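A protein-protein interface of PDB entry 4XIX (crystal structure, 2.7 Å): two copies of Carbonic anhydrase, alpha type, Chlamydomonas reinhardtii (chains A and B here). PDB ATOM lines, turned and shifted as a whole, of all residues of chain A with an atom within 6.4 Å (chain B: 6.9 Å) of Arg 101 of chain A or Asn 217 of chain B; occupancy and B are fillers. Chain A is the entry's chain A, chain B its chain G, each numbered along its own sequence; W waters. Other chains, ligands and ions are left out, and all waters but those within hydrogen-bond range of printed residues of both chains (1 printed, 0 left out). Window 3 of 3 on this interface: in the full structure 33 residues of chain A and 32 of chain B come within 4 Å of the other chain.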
ATOM      1  N   ASN A  29     -12.013  24.177  19.348  1.00  0.00           N
ATOM      2  CA  ASN A  29     -13.270  23.900  18.701  1.00  0.00           C
ATOM      3  C   ASN A  29     -13.049  23.406  17.271  1.00  0.00           C
ATOM      4  O   ASN A  29     -12.110  23.820  16.608  1.00  0.00           O
ATOM      5  CB  ASN A  29     -14.142  25.131  18.678  1.00  0.00           C
ATOM      6  CG  ASN A  29     -15.490  24.852  18.057  1.00  0.00           C
ATOM      7  OD1 ASN A  29     -16.184  23.909  18.454  1.00  0.00           O
ATOM      8  ND2 ASN A  29     -15.849  25.635  17.038  1.00  0.00           N
ATOM      9  N   SER A  94     -15.917  15.408  26.569  1.00  0.00           N
ATOM     10  CA  SER A  94     -14.905  15.430  25.511  1.00  0.00           C
ATOM     11  C   SER A  94     -14.131  16.730  25.655  1.00  0.00           C
ATOM     12  O   SER A  94     -14.565  17.626  26.380  1.00  0.00           O
ATOM     13  CB  SER A  94     -15.528  15.268  24.119  1.00  0.00           C
ATOM     14  OG  SER A  94     -16.278  16.389  23.676  1.00  0.00           O
ATOM     15  N   HIS A  96     -12.168  18.269  22.863  1.00  0.00           N
ATOM     16  CA  HIS A  96     -12.535  18.985  21.681  1.00  0.00           C
ATOM     17  C   HIS A  96     -14.044  19.177  21.711  1.00  0.00           C
ATOM     18  O   HIS A  96     -14.758  18.391  22.336  1.00  0.00           O
ATOM     19  CB  HIS A  96     -12.088  18.195  20.446  1.00  0.00           C
ATOM     20  CG  HIS A  96     -10.598  18.163  20.282  1.00  0.00           C
ATOM     21  ND1 HIS A  96      -9.793  17.314  21.006  1.00  0.00           N
ATOM     22  CD2 HIS A  96      -9.765  18.929  19.536  1.00  0.00           C
ATOM     23  CE1 HIS A  96      -8.526  17.534  20.688  1.00  0.00           C
ATOM     24  NE2 HIS A  96      -8.484  18.515  19.806  1.00  0.00           N
ATOM     25  N   ALA A  97     -14.514  20.229  21.052  1.00  0.00           N
ATOM     26  CA  ALA A  97     -15.921  20.369  20.730  1.00  0.00           C
ATOM     27  C   ALA A  97     -16.108  20.363  19.216  1.00  0.00           C
ATOM     28  O   ALA A  97     -15.171  20.608  18.472  1.00  0.00           O
ATOM     29  CB  ALA A  97     -16.438  21.637  21.279  1.00  0.00           C
ATOM     30  N   MET A  98     -17.323  20.079  18.766  1.00  0.00           N
ATOM     31  CA  MET A  98     -17.691  20.224  17.364  1.00  0.00           C
ATOM     32  C   MET A  98     -18.818  21.255  17.305  1.00  0.00           C
ATOM     33  O   MET A  98     -19.896  21.029  17.858  1.00  0.00           O
ATOM     34  CB  MET A  98     -18.200  18.901  16.787  1.00  0.00           C
ATOM     35  CG  MET A  98     -17.557  17.641  17.326  1.00  0.00           C
ATOM     36  SD  MET A  98     -16.205  17.051  16.307  1.00  0.00           S
ATOM     37  CE  MET A  98     -15.173  16.364  17.604  1.00  0.00           C
ATOM     38  N   ASP A  99     -18.584  22.383  16.644  1.00  0.00           N
ATOM     39  CA  ASP A  99     -19.568  23.471  16.614  1.00  0.00           C
ATOM     40  C   ASP A  99     -19.993  23.892  18.036  1.00  0.00           C
ATOM     41  O   ASP A  99     -21.169  24.088  18.319  1.00  0.00           O
ATOM     42  CB  ASP A  99     -20.787  23.070  15.789  1.00  0.00           C
ATOM     43  CG  ASP A  99     -20.511  23.079  14.281  1.00  0.00           C
ATOM     44  OD1 ASP A  99     -19.562  23.794  13.847  1.00  0.00           O
ATOM     45  OD2 ASP A  99     -21.256  22.386  13.534  1.00  0.00           O
ATOM     46  N   GLY A 100     -19.003  23.977  18.918  1.00  0.00           N
ATOM     47  CA  GLY A 100     -19.197  24.426  20.262  1.00  0.00           C
ATOM     48  C   GLY A 100     -19.694  23.401  21.260  1.00  0.00           C
ATOM     49  O   GLY A 100     -19.761  23.729  22.456  1.00  0.00           O
ATOM     50  N   ARG A 101     -20.043  22.191  20.809  1.00  0.00           N
ATOM     51  CA  ARG A 101     -20.670  21.205  21.698  1.00  0.00           C
ATOM     52  C   ARG A 101     -19.746  20.036  22.007  1.00  0.00           C
ATOM     53  O   ARG A 101     -19.192  19.425  21.096  1.00  0.00           O
ATOM     54  CB  ARG A 101     -21.954  20.655  21.088  1.00  0.00           C
ATOM     55  CG  ARG A 101     -22.794  21.676  20.379  1.00  0.00           C
ATOM     56  CD  ARG A 101     -24.225  21.189  20.125  1.00  0.00           C
ATOM     57  NE  ARG A 101     -25.173  22.292  20.293  1.00  0.00           N
ATOM     58  CZ  ARG A 101     -26.494  22.157  20.399  1.00  0.00           C
ATOM     59  NH1 ARG A 101     -27.052  20.950  20.338  1.00  0.00           N
ATOM     60  NH2 ARG A 101     -27.256  23.236  20.565  1.00  0.00           N
ATOM     61  N   ARG A 102     -19.603  19.719  23.294  1.00  0.00           N
ATOM     62  CA  ARG A 102     -18.764  18.614  23.751  1.00  0.00           C
ATOM     63  C   ARG A 102     -19.563  17.336  23.921  1.00  0.00           C
ATOM     64  O   ARG A 102     -20.749  17.378  24.163  1.00  0.00           O
ATOM     65  CB  ARG A 102     -18.071  18.964  25.056  1.00  0.00           C
ATOM     66  CG  ARG A 102     -16.997  19.957  24.881  1.00  0.00           C
ATOM     67  CD  ARG A 102     -16.315  20.223  26.171  1.00  0.00           C
ATOM     68  NE  ARG A 102     -14.947  20.660  25.944  1.00  0.00           N
ATOM     69  CZ  ARG A 102     -14.182  21.254  26.857  1.00  0.00           C
ATOM     70  NH1 ARG A 102     -14.651  21.494  28.069  1.00  0.00           N
ATOM     71  NH2 ARG A 102     -12.940  21.611  26.553  1.00  0.00           N
ATOM     72  N   TYR A 103     -18.906  16.196  23.743  1.00  0.00           N
ATOM     73  CA  TYR A 103     -19.555  14.902  23.858  1.00  0.00           C
ATOM     74  C   TYR A 103     -19.349  14.307  25.270  1.00  0.00           C
ATOM     75  O   TYR A 103     -18.631  14.858  26.092  1.00  0.00           O
ATOM     76  CB  TYR A 103     -18.999  13.991  22.762  1.00  0.00           C
ATOM     77  CG  TYR A 103     -19.541  14.325  21.387  1.00  0.00           C
ATOM     78  CD1 TYR A 103     -19.062  15.405  20.661  1.00  0.00           C
ATOM     79  CD2 TYR A 103     -20.548  13.553  20.813  1.00  0.00           C
ATOM     80  CE1 TYR A 103     -19.578  15.709  19.389  1.00  0.00           C
ATOM     81  CE2 TYR A 103     -21.072  13.842  19.553  1.00  0.00           C
ATOM     82  CZ  TYR A 103     -20.587  14.918  18.844  1.00  0.00           C
ATOM     83  OH  TYR A 103     -21.112  15.182  17.586  1.00  0.00           O
ATOM     84  N   MET A 125     -14.733  10.818  19.719  1.00  0.00           N
ATOM     85  CA  MET A 125     -15.806  11.209  20.612  1.00  0.00           C
ATOM     86  C   MET A 125     -16.617   9.985  21.021  1.00  0.00           C
ATOM     87  O   MET A 125     -16.963   9.154  20.191  1.00  0.00           O
ATOM     88  CB  MET A 125     -16.757  12.213  19.956  1.00  0.00           C
ATOM     89  CG  MET A 125     -16.118  13.471  19.412  1.00  0.00           C
ATOM     90  SD  MET A 125     -15.240  14.562  20.564  1.00  0.00           S
ATOM     91  CE  MET A 125     -13.584  13.988  20.234  1.00  0.00           C
ATOM     92  N   GLU B 146     -34.512  25.887  27.621  1.00  0.00           N
ATOM     93  CA  GLU B 146     -33.058  25.849  27.507  1.00  0.00           C
ATOM     94  C   GLU B 146     -32.430  27.227  27.579  1.00  0.00           C
ATOM     95  O   GLU B 146     -31.254  27.348  27.868  1.00  0.00           O
ATOM     96  CB  GLU B 146     -32.660  25.184  26.196  1.00  0.00           C
ATOM     97  CG  GLU B 146     -33.056  23.716  26.133  1.00  0.00           C
ATOM     98  CD  GLU B 146     -32.264  22.826  27.115  1.00  0.00           C
ATOM     99  OE1 GLU B 146     -32.892  22.011  27.851  1.00  0.00           O
ATOM    100  OE2 GLU B 146     -31.009  22.936  27.137  1.00  0.00           O
ATOM    101  N   MET B 211     -27.033  16.308  33.693  1.00  0.00           N
ATOM    102  CA  MET B 211     -25.687  16.910  33.594  1.00  0.00           C
ATOM    103  C   MET B 211     -25.530  17.679  32.288  1.00  0.00           C
ATOM    104  O   MET B 211     -24.816  18.689  32.217  1.00  0.00           O
ATOM    105  CB  MET B 211     -24.634  15.846  33.660  1.00  0.00           C
ATOM    106  CG  MET B 211     -24.560  15.219  35.001  1.00  0.00           C
ATOM    107  SD  MET B 211     -23.309  13.924  35.022  1.00  0.00           S
ATOM    108  CE  MET B 211     -21.835  14.948  34.942  1.00  0.00           C
ATOM    109  N   ARG B 212     -26.234  17.205  31.267  1.00  0.00           N
ATOM    110  CA  ARG B 212     -26.301  17.908  30.009  1.00  0.00           C
ATOM    111  C   ARG B 212     -27.028  19.204  30.123  1.00  0.00           C
ATOM    112  O   ARG B 212     -26.560  20.208  29.636  1.00  0.00           O
ATOM    113  CB  ARG B 212     -26.976  17.039  28.949  1.00  0.00           C
ATOM    114  CG  ARG B 212     -26.943  17.611  27.549  1.00  0.00           C
ATOM    115  CD  ARG B 212     -25.590  17.568  26.960  1.00  0.00           C
ATOM    116  NE  ARG B 212     -25.625  18.115  25.614  1.00  0.00           N
ATOM    117  CZ  ARG B 212     -24.622  18.040  24.754  1.00  0.00           C
ATOM    118  NH1 ARG B 212     -23.489  17.434  25.088  1.00  0.00           N
ATOM    119  NH2 ARG B 212     -24.763  18.577  23.560  1.00  0.00           N
ATOM    120  N   PHE B 213     -28.201  19.191  30.740  1.00  0.00           N
ATOM    121  CA  PHE B 213     -28.888  20.453  31.031  1.00  0.00           C
ATOM    122  C   PHE B 213     -28.023  21.423  31.843  1.00  0.00           C
ATOM    123  O   PHE B 213     -27.925  22.588  31.493  1.00  0.00           O
ATOM    124  CB  PHE B 213     -30.173  20.192  31.771  1.00  0.00           C
ATOM    125  CG  PHE B 213     -31.010  21.419  31.977  1.00  0.00           C
ATOM    126  CD1 PHE B 213     -30.795  22.245  33.075  1.00  0.00           C
ATOM    127  CD2 PHE B 213     -32.019  21.743  31.075  1.00  0.00           C
ATOM    128  CE1 PHE B 213     -31.568  23.376  33.260  1.00  0.00           C
ATOM    129  CE2 PHE B 213     -32.797  22.857  31.261  1.00  0.00           C
ATOM    130  CZ  PHE B 213     -32.581  23.680  32.359  1.00  0.00           C
ATOM    131  N   VAL B 214     -27.361  20.937  32.890  1.00  0.00           N
ATOM    132  CA  VAL B 214     -26.486  21.795  33.679  1.00  0.00           C
ATOM    133  C   VAL B 214     -25.422  22.417  32.816  1.00  0.00           C
ATOM    134  O   VAL B 214     -24.953  23.500  33.095  1.00  0.00           O
ATOM    135  CB  VAL B 214     -25.796  21.022  34.815  1.00  0.00           C
ATOM    136  CG1 VAL B 214     -24.826  21.910  35.593  1.00  0.00           C
ATOM    137  CG2 VAL B 214     -26.838  20.434  35.756  1.00  0.00           C
ATOM    138  N   GLY B 215     -25.020  21.707  31.768  1.00  0.00           N
ATOM    139  CA  GLY B 215     -24.002  22.209  30.870  1.00  0.00           C
ATOM    140  C   GLY B 215     -24.571  22.972  29.684  1.00  0.00           C
ATOM    141  O   GLY B 215     -24.038  22.832  28.589  1.00  0.00           O
ATOM    142  N   ASP B 216     -25.647  23.741  29.867  1.00  0.00           N
ATOM    143  CA  ASP B 216     -26.173  24.574  28.775  1.00  0.00           C
ATOM    144  C   ASP B 216     -26.376  23.762  27.472  1.00  0.00           C
ATOM    145  O   ASP B 216     -26.264  24.285  26.374  1.00  0.00           O
ATOM    146  CB  ASP B 216     -25.202  25.731  28.480  1.00  0.00           C
ATOM    147  CG  ASP B 216     -25.392  26.929  29.385  1.00  0.00           C
ATOM    148  OD1 ASP B 216     -26.086  26.812  30.423  1.00  0.00           O
ATOM    149  OD2 ASP B 216     -24.823  28.002  29.049  1.00  0.00           O
ATOM    150  N   ASN B 217     -26.638  22.478  27.587  1.00  0.00           N
ATOM    151  CA  ASN B 217     -26.914  21.679  26.408  1.00  0.00           C
ATOM    152  C   ASN B 217     -25.782  21.765  25.388  1.00  0.00           C
ATOM    153  O   ASN B 217     -26.008  21.795  24.176  1.00  0.00           O
ATOM    154  CB  ASN B 217     -28.244  22.092  25.792  1.00  0.00           C
ATOM    155  CG  ASN B 217     -28.874  20.972  24.951  1.00  0.00           C
ATOM    156  OD1 ASN B 217     -28.350  19.850  24.889  1.00  0.00           O
ATOM    157  ND2 ASN B 217     -29.994  21.280  24.286  1.00  0.00           N
ATOM    158  N   LYS B 218     -24.562  21.829  25.912  1.00  0.00           N
ATOM    159  CA  LYS B 218     -23.375  21.842  25.083  1.00  0.00           C
ATOM    160  C   LYS B 218     -22.201  21.149  25.758  1.00  0.00           C
ATOM    161  O   LYS B 218     -21.134  21.085  25.187  1.00  0.00           O
ATOM    162  CB  LYS B 218     -22.981  23.272  24.673  1.00  0.00           C
ATOM    163  CG  LYS B 218     -22.830  24.215  25.809  1.00  0.00           C
ATOM    164  CD  LYS B 218     -21.686  25.202  25.645  1.00  0.00           C
ATOM    165  CE  LYS B 218     -21.712  26.207  26.800  1.00  0.00           C
ATOM    166  NZ  LYS B 218     -20.484  27.084  26.850  1.00  0.00           N
ATOM    167  N   THR B 219     -22.366  20.662  26.982  1.00  0.00           N
ATOM    168  CA  THR B 219     -21.278  19.934  27.667  1.00  0.00           C
ATOM    169  C   THR B 219     -21.932  19.132  28.792  1.00  0.00           C
ATOM    170  O   THR B 219     -23.154  19.015  28.820  1.00  0.00           O
ATOM    171  CB  THR B 219     -20.167  20.891  28.205  1.00  0.00           C
ATOM    172  OG1 THR B 219     -18.976  20.170  28.502  1.00  0.00           O
ATOM    173  CG2 THR B 219     -20.633  21.627  29.454  1.00  0.00           C
HETATM  174  O   HOH W   1     -18.725  22.946  25.200  1.00  0.00           O
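O of Lys 218 of chain B is in hydrogen-bond range of N of Arg 102 of chain A, at 2.8 Å.
O of Arg 102 of chain A sits at hydrogen-bond distance from NH1 of Arg 212 of chain B.
Among the printed residues, pairs that only touch across the chains: Arg 101 of chain A with Lys 218 of chain B (3.5 Å), Arg 102 of chain A with Thr 219 of chain B (3.5 Å), Arg 101 of chain A with Asn 217 of chain B (3.8 Å) and Gly 100 of chain A with Lys 218 of chain B (3.9 Å).
Water W1 bridges O of Gly 100 of chain A (3.0 Å) and O of Lys 218 of chain B (3.0 Å).
Among the printed residues, no Asp or Glu carboxylate lies within 4 Å of a Lys or Arg side-chain nitrogen of the other chain.
O of Arg 212 of chain B sits at hydrogen-bond distance from N of Asn 217 of chain B (3.1 Å).
The side-chain amide nitrogen of Asn 217 of chain B sits close to the side-chain carboxylate of Glu 146 of chain B (3.4 Å).
The side-chain amide oxygen of Asn 29 of chain A lies within hydrogen-bond range of the backbone NH of Gly 100 of chain A, at 2.9 Å.
O of Ser 94 of chain A is in hydrogen-bond range of NE of Arg 102 of chain A, at 3.1 Å.
No position is printed for both chains.
Gly 100 of chain A touches one residue of chain B.
Of chain B, only Asn 217 (3.8 Å) and Lys 218 (3.5 Å) come within 4 Å of Arg 101 of chain A.
Printed residues of chain B within 4 Å of Arg 102 of chain A: Arg 212, Lys 218 and Thr 219.
Printed residues of chain A within 4 Å of Arg 212 of chain B: Arg 102 (2.9 Å).
Of chain A, only Arg 101 comes within 4 Å of Asn 217 of chain B.
Printed residues of chain A within 4 Å of Lys 218 of chain B: Gly 100 (3.9 Å), Arg 101 (3.5 Å) and Arg 102 (2.8 Å).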
